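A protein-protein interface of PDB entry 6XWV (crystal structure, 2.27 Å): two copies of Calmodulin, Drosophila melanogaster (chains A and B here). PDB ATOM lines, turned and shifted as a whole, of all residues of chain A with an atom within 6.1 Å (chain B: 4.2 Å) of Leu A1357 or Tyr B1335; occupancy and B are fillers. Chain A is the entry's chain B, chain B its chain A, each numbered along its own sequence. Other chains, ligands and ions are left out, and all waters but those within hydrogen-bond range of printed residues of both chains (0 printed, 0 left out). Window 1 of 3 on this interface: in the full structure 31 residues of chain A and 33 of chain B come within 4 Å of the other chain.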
ATOM      1  N   LYS A1355     -24.535 -14.961  11.586  1.00  0.00           N
ATOM      2  CA  LYS A1355     -24.145 -14.832  10.191  1.00  0.00           C
ATOM      3  C   LYS A1355     -25.393 -14.955   9.327  1.00  0.00           C
ATOM      4  O   LYS A1355     -26.198 -15.874   9.514  1.00  0.00           O
ATOM      5  CB  LYS A1355     -23.118 -15.894   9.794  1.00  0.00           C
ATOM      6  CG  LYS A1355     -21.673 -15.558  10.155  1.00  0.00           C
ATOM      7  CD  LYS A1355     -20.703 -16.512   9.456  1.00  0.00           C
ATOM      8  CE  LYS A1355     -19.394 -16.643  10.218  1.00  0.00           C
ATOM      9  NZ  LYS A1355     -19.612 -17.112  11.615  1.00  0.00           N
ATOM     10  N   LEU A1356     -25.557 -14.023   8.392  1.00  0.00           N
ATOM     11  CA  LEU A1356     -26.665 -14.028   7.446  1.00  0.00           C
ATOM     12  C   LEU A1356     -26.109 -14.248   6.051  1.00  0.00           C
ATOM     13  O   LEU A1356     -25.349 -13.412   5.548  1.00  0.00           O
ATOM     14  CB  LEU A1356     -27.450 -12.720   7.493  1.00  0.00           C
ATOM     15  CG  LEU A1356     -28.168 -12.395   8.796  1.00  0.00           C
ATOM     16  CD1 LEU A1356     -28.625 -10.927   8.833  1.00  0.00           C
ATOM     17  CD2 LEU A1356     -29.341 -13.336   9.009  1.00  0.00           C
ATOM     18  N   LEU A1357     -26.523 -15.337   5.414  1.00  0.00           N
ATOM     19  CA  LEU A1357     -26.071 -15.679   4.075  1.00  0.00           C
ATOM     20  C   LEU A1357     -27.278 -15.758   3.156  1.00  0.00           C
ATOM     21  O   LEU A1357     -28.254 -16.448   3.468  1.00  0.00           O
ATOM     22  CB  LEU A1357     -25.309 -17.012   4.088  1.00  0.00           C
ATOM     23  CG  LEU A1357     -24.927 -17.651   2.751  1.00  0.00           C
ATOM     24  CD1 LEU A1357     -23.882 -16.818   2.037  1.00  0.00           C
ATOM     25  CD2 LEU A1357     -24.416 -19.064   2.961  1.00  0.00           C
ATOM     26  N   VAL A1358     -27.203 -15.064   2.025  1.00  0.00           N
ATOM     27  CA  VAL A1358     -28.338 -14.941   1.116  1.00  0.00           C
ATOM     28  C   VAL A1358     -28.429 -16.203   0.262  1.00  0.00           C
ATOM     29  O   VAL A1358     -27.543 -16.480  -0.548  1.00  0.00           O
ATOM     30  CB  VAL A1358     -28.219 -13.688   0.243  1.00  0.00           C
ATOM     31  CG1 VAL A1358     -29.438 -13.547  -0.662  1.00  0.00           C
ATOM     32  CG2 VAL A1358     -28.043 -12.461   1.127  1.00  0.00           C
ATOM     33  N   GLN A1359     -29.511 -16.964   0.441  1.00  0.00           N
ATOM     34  CA  GLN A1359     -29.756 -18.141  -0.387  1.00  0.00           C
ATOM     35  C   GLN A1359     -30.343 -17.755  -1.739  1.00  0.00           C
ATOM     36  O   GLN A1359     -30.030 -18.382  -2.758  1.00  0.00           O
ATOM     37  CB  GLN A1359     -30.687 -19.108   0.340  1.00  0.00           C
ATOM     38  CG  GLN A1359     -29.989 -20.034   1.320  1.00  0.00           C
ATOM     39  CD  GLN A1359     -28.746 -20.679   0.733  1.00  0.00           C
ATOM     40  OE1 GLN A1359     -27.627 -20.417   1.176  1.00  0.00           O
ATOM     41  NE2 GLN A1359     -28.939 -21.528  -0.268  1.00  0.00           N
ATOM     42  N   PHE A1360     -31.187 -16.725  -1.769  1.00  0.00           N
ATOM     43  CA  PHE A1360     -31.803 -16.280  -3.010  1.00  0.00           C
ATOM     44  C   PHE A1360     -32.269 -14.843  -2.842  1.00  0.00           C
ATOM     45  O   PHE A1360     -32.752 -14.459  -1.772  1.00  0.00           O
ATOM     46  CB  PHE A1360     -32.989 -17.168  -3.403  1.00  0.00           C
ATOM     47  CG  PHE A1360     -33.567 -16.838  -4.749  1.00  0.00           C
ATOM     48  CD1 PHE A1360     -33.138 -17.505  -5.883  1.00  0.00           C
ATOM     49  CD2 PHE A1360     -34.534 -15.847  -4.884  1.00  0.00           C
ATOM     50  CE1 PHE A1360     -33.663 -17.199  -7.125  1.00  0.00           C
ATOM     51  CE2 PHE A1360     -35.056 -15.532  -6.121  1.00  0.00           C
ATOM     52  CZ  PHE A1360     -34.630 -16.212  -7.243  1.00  0.00           C
ATOM     53  N   LEU A1380     -26.812  -7.098   0.160  1.00  0.00           N
ATOM     54  CA  LEU A1380     -26.353  -8.476   0.036  1.00  0.00           C
ATOM     55  C   LEU A1380     -27.125  -9.155  -1.082  1.00  0.00           C
ATOM     56  O   LEU A1380     -28.362  -9.160  -1.068  1.00  0.00           O
ATOM     57  CB  LEU A1380     -26.565  -9.248   1.344  1.00  0.00           C
ATOM     58  CG  LEU A1380     -25.804  -8.839   2.604  1.00  0.00           C
ATOM     59  CD1 LEU A1380     -26.006  -9.892   3.696  1.00  0.00           C
ATOM     60  CD2 LEU A1380     -24.325  -8.641   2.315  1.00  0.00           C
ATOM     61  N   VAL A1382     -27.146 -12.860  -3.728  1.00  0.00           N
ATOM     62  CA  VAL A1382     -27.043 -14.297  -3.503  1.00  0.00           C
ATOM     63  C   VAL A1382     -25.583 -14.690  -3.309  1.00  0.00           C
ATOM     64  O   VAL A1382     -24.703 -14.306  -4.092  1.00  0.00           O
ATOM     65  CB  VAL A1382     -27.696 -15.069  -4.658  1.00  0.00           C
ATOM     66  CG1 VAL A1382     -27.080 -14.673  -5.988  1.00  0.00           C
ATOM     67  CG2 VAL A1382     -27.585 -16.576  -4.422  1.00  0.00           C
ATOM     68  N   GLY A1383     -25.318 -15.435  -2.236  1.00  0.00           N
ATOM     69  CA  GLY A1383     -23.982 -15.843  -1.890  1.00  0.00           C
ATOM     70  C   GLY A1383     -23.260 -14.892  -0.962  1.00  0.00           C
ATOM     71  O   GLY A1383     -22.266 -15.288  -0.338  1.00  0.00           O
ATOM     72  N   ASP A1384     -23.721 -13.647  -0.869  1.00  0.00           N
ATOM     73  CA  ASP A1384     -23.128 -12.687   0.048  1.00  0.00           C
ATOM     74  C   ASP A1384     -23.527 -13.009   1.482  1.00  0.00           C
ATOM     75  O   ASP A1384     -24.601 -13.560   1.747  1.00  0.00           O
ATOM     76  CB  ASP A1384     -23.554 -11.263  -0.307  1.00  0.00           C
ATOM     77  CG  ASP A1384     -23.058 -10.835  -1.671  1.00  0.00           C
ATOM     78  OD1 ASP A1384     -22.298 -11.606  -2.298  1.00  0.00           O
ATOM     79  OD2 ASP A1384     -23.422  -9.728  -2.118  1.00  0.00           O
ATOM     80  N   MET A1385     -22.642 -12.660   2.410  1.00  0.00           N
ATOM     81  CA  MET A1385     -22.830 -12.953   3.819  1.00  0.00           C
ATOM     82  C   MET A1385     -22.427 -11.741   4.643  1.00  0.00           C
ATOM     83  O   MET A1385     -21.561 -10.961   4.240  1.00  0.00           O
ATOM     84  CB  MET A1385     -22.017 -14.188   4.238  1.00  0.00           C
ATOM     85  CG  MET A1385     -22.014 -14.476   5.729  1.00  0.00           C
ATOM     86  SD  MET A1385     -20.386 -14.163   6.431  1.00  0.00           S
ATOM     87  CE  MET A1385     -19.444 -15.412   5.587  1.00  0.00           C
ATOM     88  N   ILE A1386     -23.095 -11.559   5.780  1.00  0.00           N
ATOM     89  CA  ILE A1386     -22.717 -10.543   6.753  1.00  0.00           C
ATOM     90  C   ILE A1386     -22.602 -11.195   8.123  1.00  0.00           C
ATOM     91  O   ILE A1386     -23.381 -12.092   8.466  1.00  0.00           O
ATOM     92  CB  ILE A1386     -23.710  -9.362   6.799  1.00  0.00           C
ATOM     93  CG1 ILE A1386     -23.156  -8.246   7.689  1.00  0.00           C
ATOM     94  CG2 ILE A1386     -25.075  -9.817   7.293  1.00  0.00           C
ATOM     95  CD1 ILE A1386     -23.801  -6.890   7.474  1.00  0.00           C
ATOM     96  N   VAL A1405     -34.630 -15.279   0.047  1.00  0.00           N
ATOM     97  CA  VAL A1405     -34.395 -16.264   1.094  1.00  0.00           C
ATOM     98  C   VAL A1405     -32.975 -16.099   1.605  1.00  0.00           C
ATOM     99  O   VAL A1405     -32.029 -16.025   0.812  1.00  0.00           O
ATOM    100  CB  VAL A1405     -34.629 -17.699   0.587  1.00  0.00           C
ATOM    101  CG1 VAL A1405     -34.235 -18.720   1.654  1.00  0.00           C
ATOM    102  CG2 VAL A1405     -36.080 -17.880   0.177  1.00  0.00           C
ATOM    103  N   LEU A1406     -32.824 -16.049   2.922  1.00  0.00           N
ATOM    104  CA  LEU A1406     -31.520 -15.951   3.550  1.00  0.00           C
ATOM    105  C   LEU A1406     -31.367 -17.093   4.543  1.00  0.00           C
ATOM    106  O   LEU A1406     -32.337 -17.531   5.167  1.00  0.00           O
ATOM    107  CB  LEU A1406     -31.295 -14.583   4.237  1.00  0.00           C
ATOM    108  CG  LEU A1406     -32.068 -14.003   5.430  1.00  0.00           C
ATOM    109  CD1 LEU A1406     -31.867 -14.787   6.720  1.00  0.00           C
ATOM    110  CD2 LEU A1406     -31.642 -12.557   5.631  1.00  0.00           C
ATOM    111  N   MET A1407     -30.147 -17.592   4.666  1.00  0.00           N
ATOM    112  CA  MET A1407     -29.821 -18.599   5.660  1.00  0.00           C
ATOM    113  C   MET A1407     -29.215 -17.907   6.869  1.00  0.00           C
ATOM    114  O   MET A1407     -28.286 -17.109   6.730  1.00  0.00           O
ATOM    115  CB  MET A1407     -28.840 -19.629   5.098  1.00  0.00           C
ATOM    116  CG  MET A1407     -28.171 -20.468   6.164  1.00  0.00           C
ATOM    117  SD  MET A1407     -27.034 -21.683   5.476  1.00  0.00           S
ATOM    118  CE  MET A1407     -27.966 -22.269   4.067  1.00  0.00           C
ATOM    119  N   CYS A1408     -29.729 -18.214   8.051  1.00  0.00           N
ATOM    120  CA  CYS A1408     -29.209 -17.639   9.284  1.00  0.00           C
ATOM    121  C   CYS A1408     -28.325 -18.691   9.943  1.00  0.00           C
ATOM    122  O   CYS A1408     -28.795 -19.790  10.250  1.00  0.00           O
ATOM    123  CB  CYS A1408     -30.348 -17.218  10.217  1.00  0.00           C
ATOM    124  SG  CYS A1408     -31.729 -18.398  10.312  1.00  0.00           S
ATOM    125  N   ILE A1409     -27.065 -18.342  10.204  1.00  0.00           N
ATOM    126  CA  ILE A1409     -26.071 -19.285  10.719  1.00  0.00           C
ATOM    127  C   ILE A1409     -25.571 -18.801  12.078  1.00  0.00           C
ATOM    128  O   ILE A1409     -24.947 -17.736  12.180  1.00  0.00           O
ATOM    129  CB  ILE A1409     -24.894 -19.486   9.755  1.00  0.00           C
ATOM    130  CG1 ILE A1409     -25.350 -19.917   8.359  1.00  0.00           C
ATOM    131  CG2 ILE A1409     -23.915 -20.456  10.346  1.00  0.00           C
ATOM    132  CD1 ILE A1409     -24.371 -19.577   7.261  1.00  0.00           C
ATOM    133  N   LEU B1287     -19.288 -22.369  -7.919  1.00  0.00           N
ATOM    134  CA  LEU B1287     -18.964 -23.310  -6.853  1.00  0.00           C
ATOM    135  C   LEU B1287     -18.675 -24.694  -7.420  1.00  0.00           C
ATOM    136  O   LEU B1287     -17.811 -25.418  -6.910  1.00  0.00           O
ATOM    137  CB  LEU B1287     -20.107 -23.377  -5.840  1.00  0.00           C
ATOM    138  CG  LEU B1287     -20.359 -22.154  -4.960  1.00  0.00           C
ATOM    139  CD1 LEU B1287     -21.490 -22.442  -3.979  1.00  0.00           C
ATOM    140  CD2 LEU B1287     -19.097 -21.738  -4.218  1.00  0.00           C
ATOM    141  N   LEU B1312     -14.880 -15.748  -2.638  1.00  0.00           N
ATOM    142  CA  LEU B1312     -14.798 -17.199  -2.735  1.00  0.00           C
ATOM    143  C   LEU B1312     -13.765 -17.543  -3.801  1.00  0.00           C
ATOM    144  O   LEU B1312     -14.080 -17.867  -4.947  1.00  0.00           O
ATOM    145  CB  LEU B1312     -16.166 -17.791  -3.044  1.00  0.00           C
ATOM    146  CG  LEU B1312     -17.223 -17.571  -1.957  1.00  0.00           C
ATOM    147  CD1 LEU B1312     -18.566 -18.146  -2.374  1.00  0.00           C
ATOM    148  CD2 LEU B1312     -16.764 -18.159  -0.639  1.00  0.00           C
ATOM    149  N   PHE B1314     -11.035 -20.290  -4.827  1.00  0.00           N
ATOM    150  CA  PHE B1314     -10.811 -21.706  -4.571  1.00  0.00           C
ATOM    151  C   PHE B1314      -9.323 -22.031  -4.587  1.00  0.00           C
ATOM    152  O   PHE B1314      -8.615 -21.692  -5.541  1.00  0.00           O
ATOM    153  CB  PHE B1314     -11.569 -22.550  -5.592  1.00  0.00           C
ATOM    154  CG  PHE B1314     -12.980 -22.868  -5.178  1.00  0.00           C
ATOM    155  CD1 PHE B1314     -13.257 -23.993  -4.418  1.00  0.00           C
ATOM    156  CD2 PHE B1314     -14.027 -22.026  -5.525  1.00  0.00           C
ATOM    157  CE1 PHE B1314     -14.554 -24.285  -4.030  1.00  0.00           C
ATOM    158  CE2 PHE B1314     -15.330 -22.313  -5.139  1.00  0.00           C
ATOM    159  CZ  PHE B1314     -15.592 -23.442  -4.390  1.00  0.00           C
ATOM    160  N   ASP B1321     -10.584 -28.957  -3.441  1.00  0.00           N
ATOM    161  CA  ASP B1321     -10.772 -27.526  -3.642  1.00  0.00           C
ATOM    162  C   ASP B1321     -11.501 -26.909  -2.452  1.00  0.00           C
ATOM    163  O   ASP B1321     -12.576 -27.376  -2.060  1.00  0.00           O
ATOM    164  CB  ASP B1321     -11.561 -27.269  -4.927  1.00  0.00           C
ATOM    165  CG  ASP B1321     -10.714 -27.417  -6.175  1.00  0.00           C
ATOM    166  OD1 ASP B1321      -9.473 -27.374  -6.058  1.00  0.00           O
ATOM    167  OD2 ASP B1321     -11.288 -27.569  -7.278  1.00  0.00           O
ATOM    168  N   TYR B1322     -10.920 -25.849  -1.892  1.00  0.00           N
ATOM    169  CA  TYR B1322     -11.481 -25.151  -0.742  1.00  0.00           C
ATOM    170  C   TYR B1322     -11.675 -23.676  -1.071  1.00  0.00           C
ATOM    171  O   TYR B1322     -10.795 -23.039  -1.661  1.00  0.00           O
ATOM    172  CB  TYR B1322     -10.580 -25.265   0.494  1.00  0.00           C
ATOM    173  CG  TYR B1322     -10.425 -26.661   1.046  1.00  0.00           C
ATOM    174  CD1 TYR B1322     -11.167 -27.080   2.143  1.00  0.00           C
ATOM    175  CD2 TYR B1322      -9.526 -27.555   0.481  1.00  0.00           C
ATOM    176  CE1 TYR B1322     -11.027 -28.357   2.653  1.00  0.00           C
ATOM    177  CE2 TYR B1322      -9.376 -28.833   0.987  1.00  0.00           C
ATOM    178  CZ  TYR B1322     -10.127 -29.229   2.073  1.00  0.00           C
ATOM    179  OH  TYR B1322      -9.982 -30.501   2.577  1.00  0.00           O
ATOM    180  N   ALA B1323     -12.827 -23.136  -0.676  1.00  0.00           N
ATOM    181  CA  ALA B1323     -13.098 -21.708  -0.765  1.00  0.00           C
ATOM    182  C   ALA B1323     -13.736 -21.252   0.536  1.00  0.00           C
ATOM    183  O   ALA B1323     -14.760 -21.799   0.954  1.00  0.00           O
ATOM    184  CB  ALA B1323     -14.018 -21.374  -1.948  1.00  0.00           C
ATOM    185  N   TYR B1325     -14.952 -17.789   2.997  1.00  0.00           N
ATOM    186  CA  TYR B1325     -15.206 -16.358   3.027  1.00  0.00           C
ATOM    187  C   TYR B1325     -14.126 -15.717   3.889  1.00  0.00           C
ATOM    188  O   TYR B1325     -13.691 -16.298   4.888  1.00  0.00           O
ATOM    189  CB  TYR B1325     -16.585 -16.056   3.618  1.00  0.00           C
ATOM    190  CG  TYR B1325     -17.772 -16.462   2.765  1.00  0.00           C
ATOM    191  CD1 TYR B1325     -18.199 -15.673   1.703  1.00  0.00           C
ATOM    192  CD2 TYR B1325     -18.483 -17.622   3.042  1.00  0.00           C
ATOM    193  CE1 TYR B1325     -19.293 -16.038   0.932  1.00  0.00           C
ATOM    194  CE2 TYR B1325     -19.573 -17.999   2.277  1.00  0.00           C
ATOM    195  CZ  TYR B1325     -19.977 -17.206   1.222  1.00  0.00           C
ATOM    196  OH  TYR B1325     -21.063 -17.584   0.461  1.00  0.00           O
ATOM    197  N   GLY B1334     -17.169 -21.963   4.643  1.00  0.00           N
ATOM    198  CA  GLY B1334     -16.587 -22.182   3.335  1.00  0.00           C
ATOM    199  C   GLY B1334     -17.271 -23.295   2.573  1.00  0.00           C
ATOM    200  O   GLY B1334     -18.271 -23.864   3.015  1.00  0.00           O
ATOM    201  N   TYR B1335     -16.713 -23.593   1.400  1.00  0.00           N
ATOM    202  CA  TYR B1335     -17.232 -24.632   0.522  1.00  0.00           C
ATOM    203  C   TYR B1335     -16.134 -25.627   0.170  1.00  0.00           C
ATOM    204  O   TYR B1335     -14.974 -25.246  -0.016  1.00  0.00           O
ATOM    205  CB  TYR B1335     -17.828 -24.036  -0.759  1.00  0.00           C
ATOM    206  CG  TYR B1335     -18.931 -23.041  -0.498  1.00  0.00           C
ATOM    207  CD1 TYR B1335     -20.254 -23.456  -0.376  1.00  0.00           C
ATOM    208  CD2 TYR B1335     -18.651 -21.686  -0.364  1.00  0.00           C
ATOM    209  CE1 TYR B1335     -21.267 -22.541  -0.134  1.00  0.00           C
ATOM    210  CE2 TYR B1335     -19.662 -20.768  -0.124  1.00  0.00           C
ATOM    211  CZ  TYR B1335     -20.965 -21.199  -0.010  1.00  0.00           C
ATOM    212  OH  TYR B1335     -21.964 -20.292   0.234  1.00  0.00           O
ATOM    213  N   MET B1336     -16.504 -26.900   0.077  1.00  0.00           N
ATOM    214  CA  MET B1336     -15.602 -27.957  -0.364  1.00  0.00           C
ATOM    215  C   MET B1336     -16.102 -28.482  -1.699  1.00  0.00           C
ATOM    216  O   MET B1336     -17.231 -28.974  -1.794  1.00  0.00           O
ATOM    217  CB  MET B1336     -15.522 -29.094   0.656  1.00  0.00           C
ATOM    218  CG  MET B1336     -15.061 -28.677   2.035  1.00  0.00           C
ATOM    219  SD  MET B1336     -14.858 -30.103   3.123  1.00  0.00           S
ATOM    220  CE  MET B1336     -13.531 -30.974   2.291  1.00  0.00           C
ATOM    221  N   ARG B1337     -15.272 -28.379  -2.725  1.00  0.00           N
ATOM    222  CA  ARG B1337     -15.621 -28.874  -4.044  1.00  0.00           C
ATOM    223  C   ARG B1337     -14.953 -30.226  -4.238  1.00  0.00           C
ATOM    224  O   ARG B1337     -13.719 -30.327  -4.217  1.00  0.00           O
ATOM    225  CB  ARG B1337     -15.178 -27.885  -5.121  1.00  0.00           C
ATOM    226  CG  ARG B1337     -15.602 -28.225  -6.541  1.00  0.00           C
ATOM    227  CD  ARG B1337     -14.689 -27.552  -7.552  1.00  0.00           C
ATOM    228  NE  ARG B1337     -15.018 -26.138  -7.709  1.00  0.00           N
ATOM    229  CZ  ARG B1337     -14.126 -25.177  -7.939  1.00  0.00           C
ATOM    230  NH1 ARG B1337     -12.839 -25.472  -8.052  1.00  0.00           N
ATOM    231  NH2 ARG B1337     -14.525 -23.918  -8.064  1.00  0.00           N
ATOM    232  N   GLN B1359     -24.353 -28.306  -0.660  1.00  0.00           N
ATOM    233  CA  GLN B1359     -24.704 -27.239  -1.590  1.00  0.00           C
ATOM    234  C   GLN B1359     -25.152 -27.789  -2.940  1.00  0.00           C
ATOM    235  O   GLN B1359     -26.061 -27.234  -3.567  1.00  0.00           O
ATOM    236  CB  GLN B1359     -23.509 -26.299  -1.761  1.00  0.00           C
ATOM    237  CG  GLN B1359     -23.865 -24.888  -2.218  1.00  0.00           C
ATOM    238  CD  GLN B1359     -24.808 -24.166  -1.269  1.00  0.00           C
ATOM    239  OE1 GLN B1359     -24.946 -24.535  -0.101  1.00  0.00           O
ATOM    240  NE2 GLN B1359     -25.463 -23.125  -1.771  1.00  0.00           N
ATOM    241  N   LEU B1406     -19.879 -29.069  -1.004  1.00  0.00           N
ATOM    242  CA  LEU B1406     -20.297 -29.115   0.387  1.00  0.00           C
ATOM    243  C   LEU B1406     -20.004 -27.778   1.047  1.00  0.00           C
ATOM    244  O   LEU B1406     -18.961 -27.167   0.795  1.00  0.00           O
ATOM    245  CB  LEU B1406     -19.552 -30.233   1.129  1.00  0.00           C
ATOM    246  CG  LEU B1406     -20.187 -30.878   2.358  1.00  0.00           C
ATOM    247  CD1 LEU B1406     -21.558 -31.428   2.021  1.00  0.00           C
ATOM    248  CD2 LEU B1406     -19.279 -31.980   2.897  1.00  0.00           C
ATOM    249  N   MET B1407     -20.920 -27.328   1.895  1.00  0.00           N
ATOM    250  CA  MET B1407     -20.702 -26.142   2.708  1.00  0.00           C
ATOM    251  C   MET B1407     -20.322 -26.580   4.116  1.00  0.00           C
ATOM    252  O   MET B1407     -21.027 -27.389   4.731  1.00  0.00           O
ATOM    253  CB  MET B1407     -21.946 -25.254   2.727  1.00  0.00           C
ATOM    254  CG  MET B1407     -21.838 -24.063   3.648  1.00  0.00           C
ATOM    255  SD  MET B1407     -23.189 -22.911   3.370  1.00  0.00           S
ATOM    256  CE  MET B1407     -24.272 -23.410   4.686  1.00  0.00           C
ATOM    257  N   CYS B1408     -19.207 -26.060   4.619  1.00  0.00           N
ATOM    258  CA  CYS B1408     -18.712 -26.387   5.951  1.00  0.00           C
ATOM    259  C   CYS B1408     -18.907 -25.202   6.884  1.00  0.00           C
ATOM    260  O   CYS B1408     -18.460 -24.088   6.584  1.00  0.00           O
ATOM    261  CB  CYS B1408     -17.237 -26.786   5.905  1.00  0.00           C
ATOM    262  SG  CYS B1408     -16.249 -25.771   4.793  1.00  0.00           S
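Printed residues of chain B within 4 Å of Leu A1357: Tyr B1325 (3.3 Å) and Tyr B1335 (3.9 Å). Of the printed residues of chain A, Met B1407 touches Met A1407 (3.4 Å). Of the printed residues of chain B, Met A1407 touches Met B1407. Leu B1312 touches none of the printed residues of chain A. Leu B1406 touches none of the printed residues of chain A. The nearest residue of chain A that does not touch Tyr B1335 is Gly A1383 (5.0 Å).
N of Tyr B1335 sits at hydrogen-bond distance from O of Ala B1323. The backbone NH (N) of Gly A1383 sits at hydrogen-bond distance from the backbone carbonyl oxygen (O) of Val A1358 (3.0 Å). The side-chain hydroxyl (OH) of Tyr B1325 lies within hydrogen-bond range of the side-chain hydroxyl (OH) of Tyr B1335, at 2.9 Å. N of Met A1407 is in hydrogen-bond range of O of Leu A1357, 2.5 Å away.
Met A1407 touches its own counterpart, Met B1407. Positions printed for both chains: 1359, 1406, 1407 and 1408. Of the 5 pairs that touch across the chains among the printed residues, 1 has its exchanged pair printed and touching as well.
Of the 15 printed residues of chain B, 3 touch a printed residue of chain A. Hydrophobic or aromatic side chains of chain B within 4 Å of the printed part of chain A: Tyr B1325, Tyr B1335 and Met B1407. Of the 17 printed residues of chain A, 4 touch a printed residue of chain B. Hydrophobic or aromatic side chains of chain A that line the printed part of chain B: Leu A1357, Met A1385 and Met A1407.
The side-chain hydroxyl (OH) of Tyr B1325 is in hydrogen-bond range of the backbone carbonyl oxygen (O) of Gly A1383.
Among the printed residues, merely in contact across the chains: Leu A1357 with Tyr B1325, Leu A1357 with Tyr B1335, Met A1385 with Tyr B1325 and Met A1407 with Met B1407.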
